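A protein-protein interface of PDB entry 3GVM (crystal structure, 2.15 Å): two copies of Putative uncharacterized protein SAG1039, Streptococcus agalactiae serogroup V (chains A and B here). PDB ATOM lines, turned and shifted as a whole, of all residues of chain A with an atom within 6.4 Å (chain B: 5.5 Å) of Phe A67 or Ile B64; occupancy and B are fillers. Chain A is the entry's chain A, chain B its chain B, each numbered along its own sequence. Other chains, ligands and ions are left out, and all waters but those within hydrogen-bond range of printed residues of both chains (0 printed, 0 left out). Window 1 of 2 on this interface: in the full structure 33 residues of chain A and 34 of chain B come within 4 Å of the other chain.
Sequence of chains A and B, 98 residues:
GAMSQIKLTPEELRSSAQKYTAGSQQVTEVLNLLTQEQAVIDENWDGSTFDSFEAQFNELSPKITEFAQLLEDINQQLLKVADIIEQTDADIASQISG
The side-chain amino group (NZ) of Lys A63 lies within salt-bridge range of the side-chain carboxylate (OE2) of Glu A66 (3.0 Å).
Among the printed residues, merely in contact across the chains: Val A27 with Val B30, Leu A60 with Lys B63, Leu A60 with Glu B66, Leu A60 with Phe B67, Lys A63 with Leu B60, Ile A64 with Ile B64, Ile A64 with Phe B67, Glu A66 with Leu B60, Phe A67 with Leu B31, Phe A67 with Phe B57, Phe A67 with Leu B60, Phe A67 with Ile B64, Leu A70 with Phe B57, Leu A71 with Val B30 and Leu A71 with Phe B57.
Of chain B, only Leu B31 (3.9 Å), Phe B57 (3.8 Å), Leu B60 (3.7 Å) and Ile B64 (3.5 Å) come within 4 Å of Phe A67. Of the printed residues of chain A, Ile B64 touches Ile A64 and Phe A67. Printed residues of chain A within 4 Å of Leu B60: Lys A63 (3.9 Å), Glu A66 (3.9 Å) and Phe A67 (3.7 Å). Printed residues of chain B within 4 Å of Val A27: Val B30 (3.9 Å). Of the printed residues of chain A, Phe B67 touches Leu A60 (3.7 Å) and Ile A64 (3.5 Å). Of the printed residues of chain B, Glu A66 touches Leu B60. Of the printed residues of chain A, Leu B31 touches Phe A67. The nearest printed residue of chain A that does not touch Leu B31 is Val A27 (6.1 Å).
Hydrophobic or aromatic side chains of chain B within 4 Å of the printed part of chain A: Val B30, Leu B31, Phe B57, Leu B60, Ile B64 and Phe B67. Of the 14 printed residues of chain A, 8 touch a printed residue of chain B. Along chain A the printed residues that touch a printed residue of chain B span positions 27 to 71.
Leu A60 touches Glu B66, and with the chains exchanged Glu A66 touches Leu B60. Leu A60 touches Phe B67, and with the chains exchanged Phe A67 touches Leu B60. Ile B64 touches its own counterpart, Ile A64. Ile A64 touches Phe B67, and with the chains exchanged Phe A67 touches Ile B64. Positions printed for both chains: 27, 60, 62, 63, 64, 65, 66, 67, 68 and 69.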
ATOM      1  N   SER A  24       1.701 -15.421  24.456  1.00  0.00           N
ATOM      2  CA  SER A  24       1.405 -14.329  23.521  1.00  0.00           C
ATOM      3  C   SER A  24       2.254 -13.086  23.814  1.00  0.00           C
ATOM      4  O   SER A  24       2.805 -12.457  22.914  1.00  0.00           O
ATOM      5  CB  SER A  24      -0.090 -13.958  23.613  1.00  0.00           C
ATOM      6  OG  SER A  24      -0.415 -12.894  22.736  1.00  0.00           O
ATOM      7  N   VAL A  27       6.019 -13.721  22.899  1.00  0.00           N
ATOM      8  CA  VAL A  27       6.220 -13.652  21.444  1.00  0.00           C
ATOM      9  C   VAL A  27       6.236 -12.193  20.939  1.00  0.00           C
ATOM     10  O   VAL A  27       7.101 -11.791  20.163  1.00  0.00           O
ATOM     11  CB  VAL A  27       5.153 -14.484  20.703  1.00  0.00           C
ATOM     12  CG1 VAL A  27       5.104 -14.131  19.211  1.00  0.00           C
ATOM     13  CG2 VAL A  27       5.452 -15.974  20.874  1.00  0.00           C
ATOM     14  N   LEU A  60       8.332 -12.792   7.365  1.00  0.00           N
ATOM     15  CA  LEU A  60       7.802 -13.650   8.433  1.00  0.00           C
ATOM     16  C   LEU A  60       7.093 -12.853   9.522  1.00  0.00           C
ATOM     17  O   LEU A  60       6.112 -13.309  10.101  1.00  0.00           O
ATOM     18  CB  LEU A  60       8.914 -14.490   9.055  1.00  0.00           C
ATOM     19  CG  LEU A  60       9.357 -15.702   8.243  1.00  0.00           C
ATOM     20  CD1 LEU A  60      10.700 -16.231   8.753  1.00  0.00           C
ATOM     21  CD2 LEU A  60       8.283 -16.781   8.276  1.00  0.00           C
ATOM     22  N   PRO A  62       4.804 -10.512   9.987  1.00  0.00           N
ATOM     23  CA  PRO A  62       3.345 -10.435  10.143  1.00  0.00           C
ATOM     24  C   PRO A  62       2.749 -11.759  10.642  1.00  0.00           C
ATOM     25  O   PRO A  62       1.759 -11.754  11.359  1.00  0.00           O
ATOM     26  CB  PRO A  62       2.853 -10.143   8.716  1.00  0.00           C
ATOM     27  CG  PRO A  62       3.992  -9.562   8.029  1.00  0.00           C
ATOM     28  CD  PRO A  62       5.235 -10.158   8.625  1.00  0.00           C
ATOM     29  N   LYS A  63       3.357 -12.876  10.263  1.00  0.00           N
ATOM     30  CA  LYS A  63       2.914 -14.197  10.718  1.00  0.00           C
ATOM     31  C   LYS A  63       3.113 -14.370  12.224  1.00  0.00           C
ATOM     32  O   LYS A  63       2.329 -15.044  12.903  1.00  0.00           O
ATOM     33  CB  LYS A  63       3.672 -15.299   9.958  1.00  0.00           C
ATOM     34  CG  LYS A  63       3.302 -15.400   8.496  1.00  0.00           C
ATOM     35  CD  LYS A  63       1.817 -15.683   8.390  1.00  0.00           C
ATOM     36  CE  LYS A  63       1.286 -15.577   6.965  1.00  0.00           C
ATOM     37  NZ  LYS A  63      -0.220 -15.673   6.952  1.00  0.00           N
ATOM     38  N   ILE A  64       4.178 -13.773  12.747  1.00  0.00           N
ATOM     39  CA  ILE A  64       4.452 -13.835  14.182  1.00  0.00           C
ATOM     40  C   ILE A  64       3.413 -13.042  14.975  1.00  0.00           C
ATOM     41  O   ILE A  64       2.987 -13.455  16.057  1.00  0.00           O
ATOM     42  CB  ILE A  64       5.868 -13.309  14.500  1.00  0.00           C
ATOM     43  CG1 ILE A  64       6.898 -14.036  13.626  1.00  0.00           C
ATOM     44  CG2 ILE A  64       6.182 -13.465  15.994  1.00  0.00           C
ATOM     45  CD1 ILE A  64       6.758 -15.577  13.655  1.00  0.00           C
ATOM     46  N   THR A  65       3.021 -11.885  14.454  1.00  0.00           N
ATOM     47  CA  THR A  65       1.935 -11.116  15.056  1.00  0.00           C
ATOM     48  C   THR A  65       0.618 -11.905  15.040  1.00  0.00           C
ATOM     49  O   THR A  65      -0.126 -11.890  16.012  1.00  0.00           O
ATOM     50  CB  THR A  65       1.738  -9.774  14.330  1.00  0.00           C
ATOM     51  OG1 THR A  65       2.942  -9.003  14.428  1.00  0.00           O
ATOM     52  CG2 THR A  65       0.601  -8.991  14.950  1.00  0.00           C
ATOM     53  N   GLU A  66       0.330 -12.595  13.937  1.00  0.00           N
ATOM     54  CA  GLU A  66      -0.888 -13.401  13.871  1.00  0.00           C
ATOM     55  C   GLU A  66      -0.885 -14.490  14.940  1.00  0.00           C
ATOM     56  O   GLU A  66      -1.904 -14.755  15.554  1.00  0.00           O
ATOM     57  CB  GLU A  66      -1.028 -14.081  12.513  1.00  0.00           C
ATOM     58  CG  GLU A  66      -1.212 -13.150  11.346  1.00  0.00           C
ATOM     59  CD  GLU A  66      -1.432 -13.919  10.051  1.00  0.00           C
ATOM     60  OE1 GLU A  66      -2.191 -14.916  10.088  1.00  0.00           O
ATOM     61  OE2 GLU A  66      -0.851 -13.519   9.016  1.00  0.00           O
ATOM     62  N   PHE A  67       0.264 -15.142  15.117  1.00  0.00           N
ATOM     63  CA  PHE A  67       0.445 -16.160  16.151  1.00  0.00           C
ATOM     64  C   PHE A  67       0.162 -15.566  17.514  1.00  0.00           C
ATOM     65  O   PHE A  67      -0.668 -16.079  18.277  1.00  0.00           O
ATOM     66  CB  PHE A  67       1.860 -16.778  16.077  1.00  0.00           C
ATOM     67  CG  PHE A  67       2.042 -18.038  16.915  1.00  0.00           C
ATOM     68  CD1 PHE A  67       1.263 -19.172  16.686  1.00  0.00           C
ATOM     69  CD2 PHE A  67       3.009 -18.085  17.917  1.00  0.00           C
ATOM     70  CE1 PHE A  67       1.447 -20.344  17.460  1.00  0.00           C
ATOM     71  CE2 PHE A  67       3.197 -19.245  18.696  1.00  0.00           C
ATOM     72  CZ  PHE A  67       2.407 -20.372  18.460  1.00  0.00           C
ATOM     73  N   ALA A  68       0.820 -14.461  17.827  1.00  0.00           N
ATOM     74  CA  ALA A  68       0.589 -13.808  19.112  1.00  0.00           C
ATOM     75  C   ALA A  68      -0.887 -13.472  19.355  1.00  0.00           C
ATOM     76  O   ALA A  68      -1.397 -13.636  20.470  1.00  0.00           O
ATOM     77  CB  ALA A  68       1.440 -12.538  19.242  1.00  0.00           C
ATOM     78  N   GLN A  69      -1.562 -12.982  18.322  1.00  0.00           N
ATOM     79  CA  GLN A  69      -2.975 -12.646  18.430  1.00  0.00           C
ATOM     80  C   GLN A  69      -3.846 -13.890  18.614  1.00  0.00           C
ATOM     81  O   GLN A  69      -4.842 -13.862  19.327  1.00  0.00           O
ATOM     82  CB  GLN A  69      -3.415 -11.847  17.197  1.00  0.00           C
ATOM     83  CG  GLN A  69      -2.821 -10.434  17.207  1.00  0.00           C
ATOM     84  CD  GLN A  69      -3.028  -9.691  15.903  1.00  0.00           C
ATOM     85  OE1 GLN A  69      -3.090 -10.297  14.839  1.00  0.00           O
ATOM     86  NE2 GLN A  69      -3.099  -8.363  15.979  1.00  0.00           N
ATOM     87  N   LEU A  70      -3.458 -14.980  17.962  1.00  0.00           N
ATOM     88  CA  LEU A  70      -4.169 -16.247  18.110  1.00  0.00           C
ATOM     89  C   LEU A  70      -4.081 -16.768  19.540  1.00  0.00           C
ATOM     90  O   LEU A  70      -5.092 -17.180  20.132  1.00  0.00           O
ATOM     91  CB  LEU A  70      -3.586 -17.284  17.146  1.00  0.00           C
ATOM     92  CG  LEU A  70      -4.006 -18.737  17.394  1.00  0.00           C
ATOM     93  CD1 LEU A  70      -5.513 -18.901  17.154  1.00  0.00           C
ATOM     94  CD2 LEU A  70      -3.206 -19.710  16.515  1.00  0.00           C
ATOM     95  N   LEU A  71      -2.869 -16.755  20.099  1.00  0.00           N
ATOM     96  CA  LEU A  71      -2.670 -17.245  21.464  1.00  0.00           C
ATOM     97  C   LEU A  71      -3.509 -16.444  22.457  1.00  0.00           C
ATOM     98  O   LEU A  71      -4.120 -16.999  23.376  1.00  0.00           O
ATOM     99  CB  LEU A  71      -1.186 -17.190  21.850  1.00  0.00           C
ATOM    100  CG  LEU A  71      -0.245 -17.942  20.908  1.00  0.00           C
ATOM    101  CD1 LEU A  71       1.237 -17.852  21.374  1.00  0.00           C
ATOM    102  CD2 LEU A  71      -0.691 -19.383  20.760  1.00  0.00           C
ATOM    103  N   GLU A  72      -3.530 -15.131  22.283  1.00  0.00           N
ATOM    104  CA  GLU A  72      -4.313 -14.287  23.171  1.00  0.00           C
ATOM    105  C   GLU A  72      -5.812 -14.565  23.000  1.00  0.00           C
ATOM    106  O   GLU A  72      -6.567 -14.538  23.961  1.00  0.00           O
ATOM    107  CB  GLU A  72      -4.025 -12.807  22.924  1.00  0.00           C
ATOM    108  CG  GLU A  72      -4.827 -11.889  23.842  1.00  0.00           C
ATOM    109  CD  GLU A  72      -4.512 -12.119  25.326  1.00  0.00           C
ATOM    110  OE1 GLU A  72      -3.341 -12.413  25.660  1.00  0.00           O
ATOM    111  OE2 GLU A  72      -5.439 -11.992  26.156  1.00  0.00           O
ATOM    112  N   VAL B  27      11.037 -17.872  21.555  1.00  0.00           N
ATOM    113  CA  VAL B  27       9.950 -18.156  20.630  1.00  0.00           C
ATOM    114  C   VAL B  27       9.715 -19.663  20.544  1.00  0.00           C
ATOM    115  O   VAL B  27       8.573 -20.122  20.624  1.00  0.00           O
ATOM    116  CB  VAL B  27      10.216 -17.559  19.223  1.00  0.00           C
ATOM    117  CG1 VAL B  27       9.313 -18.201  18.187  1.00  0.00           C
ATOM    118  CG2 VAL B  27      10.021 -16.043  19.262  1.00  0.00           C
ATOM    119  N   VAL B  30       7.934 -20.978  23.678  1.00  0.00           N
ATOM    120  CA  VAL B  30       6.494 -20.752  23.650  1.00  0.00           C
ATOM    121  C   VAL B  30       5.797 -21.758  22.709  1.00  0.00           C
ATOM    122  O   VAL B  30       4.776 -22.367  23.048  1.00  0.00           O
ATOM    123  CB  VAL B  30       6.152 -19.295  23.226  1.00  0.00           C
ATOM    124  CG1 VAL B  30       4.633 -19.151  22.996  1.00  0.00           C
ATOM    125  CG2 VAL B  30       6.624 -18.299  24.286  1.00  0.00           C
ATOM    126  N   LEU B  31       6.355 -21.951  21.527  1.00  0.00           N
ATOM    127  CA  LEU B  31       5.756 -22.890  20.583  1.00  0.00           C
ATOM    128  C   LEU B  31       5.626 -24.289  21.183  1.00  0.00           C
ATOM    129  O   LEU B  31       4.596 -24.950  21.041  1.00  0.00           O
ATOM    130  CB  LEU B  31       6.597 -22.973  19.309  1.00  0.00           C
ATOM    131  CG  LEU B  31       6.084 -23.929  18.225  1.00  0.00           C
ATOM    132  CD1 LEU B  31       4.684 -23.519  17.753  1.00  0.00           C
ATOM    133  CD2 LEU B  31       7.070 -23.969  17.055  1.00  0.00           C
ATOM    134  N   PHE B  57      -3.659 -22.697  14.656  1.00  0.00           N
ATOM    135  CA  PHE B  57      -2.396 -22.935  15.352  1.00  0.00           C
ATOM    136  C   PHE B  57      -1.485 -23.798  14.491  1.00  0.00           C
ATOM    137  O   PHE B  57      -0.303 -23.478  14.332  1.00  0.00           O
ATOM    138  CB  PHE B  57      -2.655 -23.581  16.722  1.00  0.00           C
ATOM    139  CG  PHE B  57      -1.415 -23.751  17.596  1.00  0.00           C
ATOM    140  CD1 PHE B  57      -0.504 -24.769  17.355  1.00  0.00           C
ATOM    141  CD2 PHE B  57      -1.209 -22.933  18.692  1.00  0.00           C
ATOM    142  CE1 PHE B  57       0.602 -24.953  18.182  1.00  0.00           C
ATOM    143  CE2 PHE B  57      -0.103 -23.109  19.531  1.00  0.00           C
ATOM    144  CZ  PHE B  57       0.809 -24.113  19.269  1.00  0.00           C
ATOM    145  N   LEU B  60       0.037 -21.882  11.448  1.00  0.00           N
ATOM    146  CA  LEU B  60       1.100 -20.927  11.770  1.00  0.00           C
ATOM    147  C   LEU B  60       2.381 -21.579  12.297  1.00  0.00           C
ATOM    148  O   LEU B  60       3.473 -21.057  12.089  1.00  0.00           O
ATOM    149  CB  LEU B  60       0.604 -19.886  12.771  1.00  0.00           C
ATOM    150  CG  LEU B  60      -0.411 -18.888  12.202  1.00  0.00           C
ATOM    151  CD1 LEU B  60      -1.064 -18.083  13.311  1.00  0.00           C
ATOM    152  CD2 LEU B  60       0.235 -17.976  11.157  1.00  0.00           C
ATOM    153  N   SER B  61       2.240 -22.711  12.985  1.00  0.00           N
ATOM    154  CA  SER B  61       3.379 -23.396  13.613  1.00  0.00           C
ATOM    155  C   SER B  61       4.666 -23.470  12.765  1.00  0.00           C
ATOM    156  O   SER B  61       5.748 -23.126  13.247  1.00  0.00           O
ATOM    157  CB  SER B  61       2.965 -24.804  14.091  1.00  0.00           C
ATOM    158  OG  SER B  61       4.044 -25.461  14.742  1.00  0.00           O
ATOM    159  N   PRO B  62       4.564 -23.923  11.501  1.00  0.00           N
ATOM    160  CA  PRO B  62       5.771 -24.009  10.657  1.00  0.00           C
ATOM    161  C   PRO B  62       6.449 -22.662  10.412  1.00  0.00           C
ATOM    162  O   PRO B  62       7.672 -22.632  10.250  1.00  0.00           O
ATOM    163  CB  PRO B  62       5.258 -24.575   9.321  1.00  0.00           C
ATOM    164  CG  PRO B  62       3.902 -25.125   9.614  1.00  0.00           C
ATOM    165  CD  PRO B  62       3.357 -24.410  10.815  1.00  0.00           C
ATOM    166  N   LYS B  63       5.679 -21.576  10.368  1.00  0.00           N
ATOM    167  CA  LYS B  63       6.257 -20.234  10.211  1.00  0.00           C
ATOM    168  C   LYS B  63       6.979 -19.813  11.485  1.00  0.00           C
ATOM    169  O   LYS B  63       7.960 -19.073  11.444  1.00  0.00           O
ATOM    170  CB  LYS B  63       5.170 -19.195   9.909  1.00  0.00           C
ATOM    171  CG  LYS B  63       4.262 -19.543   8.742  1.00  0.00           C
ATOM    172  CD  LYS B  63       5.028 -19.501   7.448  1.00  0.00           C
ATOM    173  CE  LYS B  63       4.088 -19.505   6.253  1.00  0.00           C
ATOM    174  NZ  LYS B  63       3.290 -20.763   6.191  1.00  0.00           N
ATOM    175  N   ILE B  64       6.474 -20.263  12.625  1.00  0.00           N
ATOM    176  CA  ILE B  64       7.083 -19.904  13.891  1.00  0.00           C
ATOM    177  C   ILE B  64       8.442 -20.599  13.971  1.00  0.00           C
ATOM    178  O   ILE B  64       9.432 -20.014  14.399  1.00  0.00           O
ATOM    179  CB  ILE B  64       6.197 -20.304  15.077  1.00  0.00           C
ATOM    180  CG1 ILE B  64       4.773 -19.756  14.878  1.00  0.00           C
ATOM    181  CG2 ILE B  64       6.820 -19.806  16.387  1.00  0.00           C
ATOM    182  CD1 ILE B  64       4.737 -18.248  14.713  1.00  0.00           C
ATOM    183  N   THR B  65       8.483 -21.845  13.515  1.00  0.00           N
ATOM    184  CA  THR B  65       9.731 -22.587  13.423  1.00  0.00           C
ATOM    185  C   THR B  65      10.721 -21.912  12.459  1.00  0.00           C
ATOM    186  O   THR B  65      11.904 -21.810  12.766  1.00  0.00           O
ATOM    187  CB  THR B  65       9.460 -24.046  13.022  1.00  0.00           C
ATOM    188  OG1 THR B  65       8.752 -24.688  14.090  1.00  0.00           O
ATOM    189  CG2 THR B  65      10.754 -24.795  12.771  1.00  0.00           C
ATOM    190  N   GLU B  66      10.241 -21.436  11.306  1.00  0.00           N
ATOM    191  CA  GLU B  66      11.119 -20.759  10.348  1.00  0.00           C
ATOM    192  C   GLU B  66      11.691 -19.470  10.924  1.00  0.00           C
ATOM    193  O   GLU B  66      12.866 -19.172  10.751  1.00  0.00           O
ATOM    194  CB  GLU B  66      10.374 -20.432   9.059  1.00  0.00           C
ATOM    195  CG  GLU B  66       9.937 -21.637   8.277  1.00  0.00           C
ATOM    196  CD  GLU B  66       9.020 -21.240   7.134  1.00  0.00           C
ATOM    197  OE1 GLU B  66       9.303 -20.192   6.507  1.00  0.00           O
ATOM    198  OE2 GLU B  66       8.020 -21.962   6.886  1.00  0.00           O
ATOM    199  N   PHE B  67      10.835 -18.715  11.601  1.00  0.00           N
ATOM    200  CA  PHE B  67      11.229 -17.470  12.246  1.00  0.00           C
ATOM    201  C   PHE B  67      12.290 -17.697  13.316  1.00  0.00           C
ATOM    202  O   PHE B  67      13.302 -17.005  13.335  1.00  0.00           O
ATOM    203  CB  PHE B  67      10.001 -16.774  12.835  1.00  0.00           C
ATOM    204  CG  PHE B  67      10.274 -15.395  13.381  1.00  0.00           C
ATOM    205  CD1 PHE B  67      10.145 -15.134  14.741  1.00  0.00           C
ATOM    206  CD2 PHE B  67      10.630 -14.351  12.529  1.00  0.00           C
ATOM    207  CE1 PHE B  67      10.378 -13.863  15.255  1.00  0.00           C
ATOM    208  CE2 PHE B  67      10.855 -13.078  13.028  1.00  0.00           C
ATOM    209  CZ  PHE B  67      10.731 -12.826  14.395  1.00  0.00           C
ATOM    210  N   ALA B  68      12.076 -18.675  14.191  1.00  0.00           N
ATOM    211  CA  ALA B  68      13.061 -18.975  15.237  1.00  0.00           C
ATOM    212  C   ALA B  68      14.415 -19.341  14.646  1.00  0.00           C
ATOM    213  O   ALA B  68      15.463 -18.959  15.170  1.00  0.00           O
ATOM    214  CB  ALA B  68      12.580 -20.087  16.124  1.00  0.00           C
ATOM    215  N   GLN B  69      14.386 -20.092  13.554  1.00  0.00           N
ATOM    216  CA  GLN B  69      15.617 -20.480  12.887  1.00  0.00           C
ATOM    217  C   GLN B  69      16.294 -19.276  12.203  1.00  0.00           C
ATOM    218  O   GLN B  69      17.520 -19.155  12.224  1.00  0.00           O
ATOM    219  CB  GLN B  69      15.333 -21.584  11.869  1.00  0.00           C
ATOM    220  CG  GLN B  69      16.585 -22.165  11.237  1.00  0.00           C
ATOM    221  CD  GLN B  69      17.537 -22.751  12.260  1.00  0.00           C
ATOM    222  OE1 GLN B  69      17.144 -23.542  13.112  1.00  0.00           O
ATOM    223  NE2 GLN B  69      18.806 -22.378  12.164  1.00  0.00           N
